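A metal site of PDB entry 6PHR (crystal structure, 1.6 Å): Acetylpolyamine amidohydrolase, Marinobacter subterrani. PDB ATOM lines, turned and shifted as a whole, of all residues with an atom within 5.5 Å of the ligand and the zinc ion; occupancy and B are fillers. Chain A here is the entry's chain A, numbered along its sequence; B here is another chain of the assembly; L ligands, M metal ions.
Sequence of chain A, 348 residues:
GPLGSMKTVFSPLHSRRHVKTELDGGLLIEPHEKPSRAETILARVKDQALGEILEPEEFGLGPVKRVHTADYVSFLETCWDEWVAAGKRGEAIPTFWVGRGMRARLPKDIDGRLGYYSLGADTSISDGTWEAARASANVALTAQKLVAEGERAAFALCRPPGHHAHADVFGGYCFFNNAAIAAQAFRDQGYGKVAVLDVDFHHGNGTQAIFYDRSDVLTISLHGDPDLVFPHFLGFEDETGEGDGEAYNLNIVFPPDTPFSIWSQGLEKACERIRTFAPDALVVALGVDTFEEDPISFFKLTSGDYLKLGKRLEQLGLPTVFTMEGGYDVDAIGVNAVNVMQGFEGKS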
ATOM      1  N   GLU A  22      18.513  -5.391 -14.095  1.00  0.00           N
ATOM      2  CA  GLU A  22      18.283  -5.217 -12.659  1.00  0.00           C
ATOM      3  C   GLU A  22      17.187  -4.168 -12.475  1.00  0.00           C
ATOM      4  O   GLU A  22      17.283  -3.064 -13.030  1.00  0.00           O
ATOM      5  CB  GLU A  22      19.558  -4.786 -11.923  1.00  0.00           C
ATOM      6  CG  GLU A  22      19.283  -4.258 -10.527  1.00  0.00           C
ATOM      7  CD  GLU A  22      20.536  -4.024  -9.710  1.00  0.00           C
ATOM      8  OE1 GLU A  22      21.632  -4.441 -10.161  1.00  0.00           O
ATOM      9  OE2 GLU A  22      20.409  -3.413  -8.632  1.00  0.00           O
ATOM     10  N   LEU A  23      16.141  -4.507 -11.734  1.00  0.00           N
ATOM     11  CA  LEU A  23      15.115  -3.526 -11.403  1.00  0.00           C
ATOM     12  C   LEU A  23      15.666  -2.480 -10.428  1.00  0.00           C
ATOM     13  O   LEU A  23      16.147  -2.825  -9.345  1.00  0.00           O
ATOM     14  CB  LEU A  23      13.897  -4.227 -10.787  1.00  0.00           C
ATOM     15  CG  LEU A  23      12.810  -3.258 -10.304  1.00  0.00           C
ATOM     16  CD1 LEU A  23      12.159  -2.556 -11.483  1.00  0.00           C
ATOM     17  CD2 LEU A  23      11.754  -3.968  -9.469  1.00  0.00           C
ATOM     18  N   ASP A  24      15.616  -1.209 -10.832  1.00  0.00           N
ATOM     19  CA  ASP A  24      16.173  -0.138 -10.019  1.00  0.00           C
ATOM     20  C   ASP A  24      15.406   1.141 -10.316  1.00  0.00           C
ATOM     21  O   ASP A  24      15.341   1.564 -11.473  1.00  0.00           O
ATOM     22  CB  ASP A  24      17.680   0.037 -10.316  1.00  0.00           C
ATOM     23  CG  ASP A  24      18.351   1.092  -9.431  1.00  0.00           C
ATOM     24  OD1 ASP A  24      18.386   2.278  -9.820  1.00  0.00           O
ATOM     25  OD2 ASP A  24      18.881   0.723  -8.357  1.00  0.00           O
ATOM     26  N   GLY A  25      14.790   1.733  -9.289  1.00  0.00           N
ATOM     27  CA  GLY A  25      14.094   2.990  -9.495  1.00  0.00           C
ATOM     28  C   GLY A  25      13.009   2.951 -10.550  1.00  0.00           C
ATOM     29  O   GLY A  25      12.805   3.937 -11.250  1.00  0.00           O
ATOM     30  N   HIS A  32      24.421  -4.020 -11.127  1.00  0.00           N
ATOM     31  CA  HIS A  32      25.612  -3.581 -10.397  1.00  0.00           C
ATOM     32  C   HIS A  32      26.570  -4.731 -10.123  1.00  0.00           C
ATOM     33  O   HIS A  32      27.795  -4.523 -10.097  1.00  0.00           O
ATOM     34  CB  HIS A  32      25.207  -2.959  -9.065  1.00  0.00           C
ATOM     35  CG  HIS A  32      24.553  -1.618  -9.173  1.00  0.00           C
ATOM     36  ND1 HIS A  32      25.263  -0.474  -9.494  1.00  0.00           N
ATOM     37  CD2 HIS A  32      23.279  -1.223  -8.973  1.00  0.00           C
ATOM     38  CE1 HIS A  32      24.448   0.565  -9.488  1.00  0.00           C
ATOM     39  NE2 HIS A  32      23.239   0.140  -9.183  1.00  0.00           N
ATOM     40  N   ASP A 122      15.436  -7.148  -7.429  1.00  0.00           N
ATOM     41  CA  ASP A 122      16.622  -6.610  -8.097  1.00  0.00           C
ATOM     42  C   ASP A 122      17.668  -7.675  -8.406  1.00  0.00           C
ATOM     43  O   ASP A 122      18.767  -7.326  -8.866  1.00  0.00           O
ATOM     44  CB  ASP A 122      17.232  -5.483  -7.262  1.00  0.00           C
ATOM     45  CG  ASP A 122      17.648  -5.935  -5.878  1.00  0.00           C
ATOM     46  OD1 ASP A 122      17.484  -7.120  -5.568  1.00  0.00           O
ATOM     47  OD2 ASP A 122      18.174  -5.097  -5.114  1.00  0.00           O
ATOM     48  N   PRO A 161      27.862 -12.894  -4.344  1.00  0.00           N
ATOM     49  CA  PRO A 161      28.007 -12.801  -2.884  1.00  0.00           C
ATOM     50  C   PRO A 161      26.943 -13.617  -2.157  1.00  0.00           C
ATOM     51  O   PRO A 161      26.058 -14.224  -2.790  1.00  0.00           O
ATOM     52  CB  PRO A 161      27.846 -11.304  -2.607  1.00  0.00           C
ATOM     53  CG  PRO A 161      26.868 -10.872  -3.711  1.00  0.00           C
ATOM     54  CD  PRO A 161      27.302 -11.660  -4.923  1.00  0.00           C
ATOM     55  N   HIS A 163      25.798 -12.818   1.733  1.00  0.00           N
ATOM     56  CA  HIS A 163      25.388 -12.549   3.113  1.00  0.00           C
ATOM     57  C   HIS A 163      23.917 -12.169   3.253  1.00  0.00           C
ATOM     58  O   HIS A 163      23.400 -12.187   4.381  1.00  0.00           O
ATOM     59  CB  HIS A 163      26.297 -11.486   3.748  1.00  0.00           C
ATOM     60  CG  HIS A 163      26.140 -10.110   3.171  1.00  0.00           C
ATOM     61  ND1 HIS A 163      26.316  -8.968   3.925  1.00  0.00           N
ATOM     62  CD2 HIS A 163      25.840  -9.696   1.917  1.00  0.00           C
ATOM     63  CE1 HIS A 163      26.101  -7.909   3.168  1.00  0.00           C
ATOM     64  NE2 HIS A 163      25.835  -8.315   1.941  1.00  0.00           N
ATOM     65  N   HIS A 164      23.205 -11.878   2.152  1.00  0.00           N
ATOM     66  CA  HIS A 164      21.776 -11.564   2.218  1.00  0.00           C
ATOM     67  C   HIS A 164      20.865 -12.782   2.060  1.00  0.00           C
ATOM     68  O   HIS A 164      19.660 -12.652   2.275  1.00  0.00           O
ATOM     69  CB  HIS A 164      21.394 -10.555   1.136  1.00  0.00           C
ATOM     70  CG  HIS A 164      21.986  -9.205   1.357  1.00  0.00           C
ATOM     71  ND1 HIS A 164      21.905  -8.540   2.561  1.00  0.00           N
ATOM     72  CD2 HIS A 164      22.720  -8.412   0.531  1.00  0.00           C
ATOM     73  CE1 HIS A 164      22.510  -7.374   2.454  1.00  0.00           C
ATOM     74  NE2 HIS A 164      23.026  -7.280   1.242  1.00  0.00           N
ATOM     75  N   GLY A 172      19.258  -9.480  -2.665  1.00  0.00           N
ATOM     76  CA  GLY A 172      20.452  -8.668  -2.463  1.00  0.00           C
ATOM     77  C   GLY A 172      21.631  -9.204  -3.241  1.00  0.00           C
ATOM     78  O   GLY A 172      22.781  -9.122  -2.783  1.00  0.00           O
ATOM     79  N   TYR A 173      21.358  -9.746  -4.420  1.00  0.00           N
ATOM     80  CA  TYR A 173      22.353 -10.300  -5.333  1.00  0.00           C
ATOM     81  C   TYR A 173      22.926 -11.629  -4.860  1.00  0.00           C
ATOM     82  O   TYR A 173      23.883 -12.129  -5.461  1.00  0.00           O
ATOM     83  CB  TYR A 173      23.527  -9.328  -5.586  1.00  0.00           C
ATOM     84  CG  TYR A 173      23.173  -7.887  -5.902  1.00  0.00           C
ATOM     85  CD1 TYR A 173      21.962  -7.545  -6.498  1.00  0.00           C
ATOM     86  CD2 TYR A 173      24.080  -6.873  -5.616  1.00  0.00           C
ATOM     87  CE1 TYR A 173      21.654  -6.215  -6.791  1.00  0.00           C
ATOM     88  CE2 TYR A 173      23.786  -5.544  -5.908  1.00  0.00           C
ATOM     89  CZ  TYR A 173      22.580  -5.224  -6.498  1.00  0.00           C
ATOM     90  OH  TYR A 173      22.291  -3.908  -6.773  1.00  0.00           O
ATOM     91  N   CYS A 174      22.350 -12.230  -3.821  1.00  0.00           N
ATOM     92  CA  CYS A 174      22.894 -13.415  -3.155  1.00  0.00           C
ATOM     93  C   CYS A 174      21.953 -14.608  -3.263  1.00  0.00           C
ATOM     94  O   CYS A 174      20.718 -14.453  -3.216  1.00  0.00           O
ATOM     95  CB  CYS A 174      23.108 -13.173  -1.675  1.00  0.00           C
ATOM     96  SG  CYS A 174      24.133 -11.751  -1.260  1.00  0.00           S
ATOM     97  N   ASP A 200      30.557  -5.522   5.327  1.00  0.00           N
ATOM     98  CA  ASP A 200      29.855  -4.968   4.188  1.00  0.00           C
ATOM     99  C   ASP A 200      28.918  -3.851   4.633  1.00  0.00           C
ATOM    100  O   ASP A 200      28.417  -3.837   5.757  1.00  0.00           O
ATOM    101  CB  ASP A 200      29.079  -6.102   3.491  1.00  0.00           C
ATOM    102  CG  ASP A 200      28.355  -5.669   2.219  1.00  0.00           C
ATOM    103  OD1 ASP A 200      27.279  -5.041   2.300  1.00  0.00           O
ATOM    104  OD2 ASP A 200      28.842  -5.978   1.122  1.00  0.00           O
ATOM    105  N   PHE A 201      28.706  -2.870   3.741  1.00  0.00           N
ATOM    106  CA  PHE A 201      27.869  -1.729   4.096  1.00  0.00           C
ATOM    107  C   PHE A 201      26.461  -2.170   4.485  1.00  0.00           C
ATOM    108  O   PHE A 201      25.833  -1.538   5.332  1.00  0.00           O
ATOM    109  CB  PHE A 201      27.798  -0.739   2.918  1.00  0.00           C
ATOM    110  CG  PHE A 201      26.697   0.300   3.049  1.00  0.00           C
ATOM    111  CD1 PHE A 201      26.892   1.443   3.828  1.00  0.00           C
ATOM    112  CD2 PHE A 201      25.474   0.127   2.405  1.00  0.00           C
ATOM    113  CE1 PHE A 201      25.918   2.385   3.965  1.00  0.00           C
ATOM    114  CE2 PHE A 201      24.465   1.084   2.540  1.00  0.00           C
ATOM    115  CZ  PHE A 201      24.696   2.228   3.327  1.00  0.00           C
ATOM    116  N   HIS A 202      25.942  -3.238   3.865  1.00  0.00           N
ATOM    117  CA  HIS A 202      24.571  -3.661   4.142  1.00  0.00           C
ATOM    118  C   HIS A 202      24.537  -4.686   5.264  1.00  0.00           C
ATOM    119  O   HIS A 202      25.512  -5.398   5.510  1.00  0.00           O
ATOM    120  CB  HIS A 202      23.937  -4.248   2.878  1.00  0.00           C
ATOM    121  CG  HIS A 202      23.925  -3.300   1.721  1.00  0.00           C
ATOM    122  ND1 HIS A 202      24.981  -3.208   0.830  1.00  0.00           N
ATOM    123  CD2 HIS A 202      23.042  -2.334   1.367  1.00  0.00           C
ATOM    124  CE1 HIS A 202      24.730  -2.237  -0.030  1.00  0.00           C
ATOM    125  NE2 HIS A 202      23.561  -1.690   0.274  1.00  0.00           N
ATOM    126  N   PHE A 230      18.539  -0.725   2.274  1.00  0.00           N
ATOM    127  CA  PHE A 230      18.440  -2.178   2.212  1.00  0.00           C
ATOM    128  C   PHE A 230      19.294  -2.817   3.308  1.00  0.00           C
ATOM    129  O   PHE A 230      20.453  -2.412   3.508  1.00  0.00           O
ATOM    130  CB  PHE A 230      18.900  -2.627   0.825  1.00  0.00           C
ATOM    131  CG  PHE A 230      18.830  -4.098   0.614  1.00  0.00           C
ATOM    132  CD1 PHE A 230      17.628  -4.689   0.180  1.00  0.00           C
ATOM    133  CD2 PHE A 230      19.945  -4.894   0.797  1.00  0.00           C
ATOM    134  CE1 PHE A 230      17.555  -6.029  -0.017  1.00  0.00           C
ATOM    135  CE2 PHE A 230      19.863  -6.262   0.593  1.00  0.00           C
ATOM    136  CZ  PHE A 230      18.676  -6.830   0.178  1.00  0.00           C
ATOM    137  N   ASP A 289      31.724  -1.906  -0.292  1.00  0.00           N
ATOM    138  CA  ASP A 289      30.776  -0.845  -0.607  1.00  0.00           C
ATOM    139  C   ASP A 289      30.637   0.158   0.533  1.00  0.00           C
ATOM    140  O   ASP A 289      29.751   1.000   0.499  1.00  0.00           O
ATOM    141  CB  ASP A 289      29.390  -1.421  -1.036  1.00  0.00           C
ATOM    142  CG  ASP A 289      28.864  -2.562  -0.148  1.00  0.00           C
ATOM    143  OD1 ASP A 289      29.451  -2.850   0.916  1.00  0.00           O
ATOM    144  OD2 ASP A 289      27.804  -3.179  -0.521  1.00  0.00           O
ATOM    145  N   ILE A 296      25.938   2.664  -4.287  1.00  0.00           N
ATOM    146  CA  ILE A 296      24.694   2.271  -3.631  1.00  0.00           C
ATOM    147  C   ILE A 296      24.909   2.217  -2.124  1.00  0.00           C
ATOM    148  O   ILE A 296      24.348   1.364  -1.427  1.00  0.00           O
ATOM    149  CB  ILE A 296      24.161   0.939  -4.177  1.00  0.00           C
ATOM    150  CG1 ILE A 296      25.162  -0.191  -3.993  1.00  0.00           C
ATOM    151  CG2 ILE A 296      23.789   1.076  -5.664  1.00  0.00           C
ATOM    152  CD1 ILE A 296      24.681  -1.499  -4.640  1.00  0.00           C
ATOM    153  N   GLU A 325      31.852 -10.081  -0.417  1.00  0.00           N
ATOM    154  CA  GLU A 325      30.443  -9.713  -0.574  1.00  0.00           C
ATOM    155  C   GLU A 325      30.293  -8.610  -1.615  1.00  0.00           C
ATOM    156  O   GLU A 325      30.630  -8.826  -2.784  1.00  0.00           O
ATOM    157  CB  GLU A 325      29.839  -9.317   0.778  1.00  0.00           C
ATOM    158  CG  GLU A 325      30.030 -10.368   1.887  1.00  0.00           C
ATOM    159  CD  GLU A 325      29.273 -11.678   1.638  1.00  0.00           C
ATOM    160  OE1 GLU A 325      28.276 -11.690   0.897  1.00  0.00           O
ATOM    161  OE2 GLU A 325      29.673 -12.706   2.223  1.00  0.00           O
ATOM    162  N   GLY A 326      29.835  -7.408  -1.204  1.00  0.00           N
ATOM    163  CA  GLY A 326      29.614  -6.299  -2.122  1.00  0.00           C
ATOM    164  C   GLY A 326      30.824  -5.388  -2.350  1.00  0.00           C
ATOM    165  O   GLY A 326      31.938  -5.652  -1.893  1.00  0.00           O
ATOM    166  N   GLY A 327      30.575  -4.275  -3.050  1.00  0.00           N
ATOM    167  CA  GLY A 327      31.579  -3.322  -3.547  1.00  0.00           C
ATOM    168  C   GLY A 327      31.308  -3.060  -5.023  1.00  0.00           C
ATOM    169  O   GLY A 327      31.505  -3.973  -5.832  1.00  0.00           O
ATOM    170  N   TYR A 328      30.854  -1.846  -5.393  1.00  0.00           N
ATOM    171  CA  TYR A 328      30.263  -1.632  -6.713  1.00  0.00           C
ATOM    172  C   TYR A 328      30.843  -0.450  -7.493  1.00  0.00           C
ATOM    173  O   TYR A 328      30.372  -0.178  -8.613  1.00  0.00           O
ATOM    174  CB  TYR A 328      28.731  -1.475  -6.577  1.00  0.00           C
ATOM    175  CG  TYR A 328      28.184  -2.713  -5.930  1.00  0.00           C
ATOM    176  CD1 TYR A 328      27.926  -2.748  -4.559  1.00  0.00           C
ATOM    177  CD2 TYR A 328      28.067  -3.889  -6.652  1.00  0.00           C
ATOM    178  CE1 TYR A 328      27.462  -3.938  -3.933  1.00  0.00           C
ATOM    179  CE2 TYR A 328      27.627  -5.077  -6.054  1.00  0.00           C
ATOM    180  CZ  TYR A 328      27.336  -5.088  -4.690  1.00  0.00           C
ATOM    181  OH  TYR A 328      26.913  -6.252  -4.107  1.00  0.00           O
ATOM    182  N   THR B  95      11.004  -2.551  -5.043  1.00  0.00           N
ATOM    183  CA  THR B  95      12.170  -3.364  -5.332  1.00  0.00           C
ATOM    184  C   THR B  95      12.465  -4.399  -4.250  1.00  0.00           C
ATOM    185  O   THR B  95      13.065  -5.432  -4.543  1.00  0.00           O
ATOM    186  CB  THR B  95      13.423  -2.504  -5.518  1.00  0.00           C
ATOM    187  OG1 THR B  95      13.104  -1.275  -6.202  1.00  0.00           O
ATOM    188  CG2 THR B  95      14.499  -3.269  -6.315  1.00  0.00           C
ATOM    189  N   PHE B  96      12.072  -4.115  -3.008  1.00  0.00           N
ATOM    190  CA  PHE B  96      12.356  -4.967  -1.853  1.00  0.00           C
ATOM    191  C   PHE B  96      11.120  -5.019  -0.990  1.00  0.00           C
ATOM    192  O   PHE B  96      10.332  -4.076  -0.979  1.00  0.00           O
ATOM    193  CB  PHE B  96      13.496  -4.418  -0.967  1.00  0.00           C
ATOM    194  CG  PHE B  96      14.479  -3.547  -1.681  1.00  0.00           C
ATOM    195  CD1 PHE B  96      15.379  -4.106  -2.565  1.00  0.00           C
ATOM    196  CD2 PHE B  96      14.543  -2.179  -1.426  1.00  0.00           C
ATOM    197  CE1 PHE B  96      16.314  -3.327  -3.210  1.00  0.00           C
ATOM    198  CE2 PHE B  96      15.485  -1.405  -2.076  1.00  0.00           C
ATOM    199  CZ  PHE B  96      16.370  -1.987  -2.980  1.00  0.00           C
HETATM  200  C1  LIG L   1      18.406  -2.167  -6.219  1.00  0.00           C
HETATM  201  C2  LIG L   1      19.764  -1.682  -5.696  1.00  0.00           C
HETATM  202  C3  LIG L   1      19.936  -2.234  -4.292  1.00  0.00           C
HETATM  203  C4  LIG L   1      20.213  -4.181  -2.952  1.00  0.00           C
HETATM  204  C5  LIG L   1      21.519  -3.969  -2.214  1.00  0.00           C
HETATM  205  C6  LIG L   1      22.438  -5.126  -2.540  1.00  0.00           C
HETATM  206  C7  LIG L   1      23.675  -5.094  -1.631  1.00  0.00           C
HETATM  207  C8  LIG L   1      24.458  -6.353  -1.975  1.00  0.00           C
HETATM  208  N1  LIG L   1      18.331  -2.008  -7.667  1.00  0.00           N
HETATM  209  N2  LIG L   1      20.257  -3.653  -4.313  1.00  0.00           N
HETATM  210  S1  LIG L   1      26.010  -6.517  -1.045  1.00  0.00           S
HETATM  211 ZN    ZN M   1      26.646  -4.593   0.323  1.00  0.00          ZN
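The zinc ion is bound by the side-chain carboxylate of Asp 289 (2.0 Å), the side-chain carboxylate of Asp 200 (2.1 Å), a ring nitrogen (ND1) of His 202 (2.2 Å) and a sulfur (S1) of the ligand (2.4 Å).
Slightly farther from the zinc ion lies OD2 of Asp 200 (2.7 Å).
Merely in contact with the ligand: His 164 (3.6 Å), Gly 172 (3.3 Å), Phe 230 (3.5 Å), Gly 326 (3.8 Å) and Phe 96 of chain B (3.8 Å).
Hydrophobic or aromatic side chains within 4 Å of the ligand: His 164, Tyr 173, His 202, Phe 230 and Phe 96 of chain B.
N of Phe 201 lies within hydrogen-bond range of OD1 of Asp 289 (2.9 Å).
N of Gly 326 sits at hydrogen-bond distance from OD2 of Asp 200 (2.9 Å).
OH of Tyr 173 is in hydrogen-bond range of OE2 of Glu 22 (2.7 Å).
OE1 of Glu 22 is in hydrogen-bond range of N of His 32.
O of Gly 172 sits at hydrogen-bond distance from SG of Cys 174, at 3.3 Å.
The side-chain carboxylate (OE1) of Glu 325 lies within hydrogen-bond range of the backbone NH (N) of His 163.
The backbone NH of His 163 sits at hydrogen-bond distance from the side-chain sulfur of Cys 174.
N of His 164 sits at hydrogen-bond distance from SG of Cys 174 (3.5 Å).
The side-chain carboxylate (OD2) of Asp 122 is in salt-bridge range of a nitrogen (N2) of the ligand, at 2.7 Å.
The side-chain carboxylate (OE2) of Glu 22 is in salt-bridge range of a nitrogen (N1) of the ligand, 2.7 Å away.
The side-chain carboxylate (OD2) of Asp 24 lies within salt-bridge range of a nitrogen (N1) of the ligand, 2.9 Å away.
The backbone carbonyl oxygen (O) of Leu 23 lies within hydrogen-bond range of a nitrogen (N1) of the ligand, 2.9 Å away.
OH of Tyr 173 is in hydrogen-bond range of N2 of the ligand (3.2 Å).
A sulfur (S1) of the ligand lies close to the side-chain hydroxyl (OH) of Tyr 328.
A sulfur (S1) of the ligand sits close to a ring nitrogen (NE2) of His 163, 3.5 Å away.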
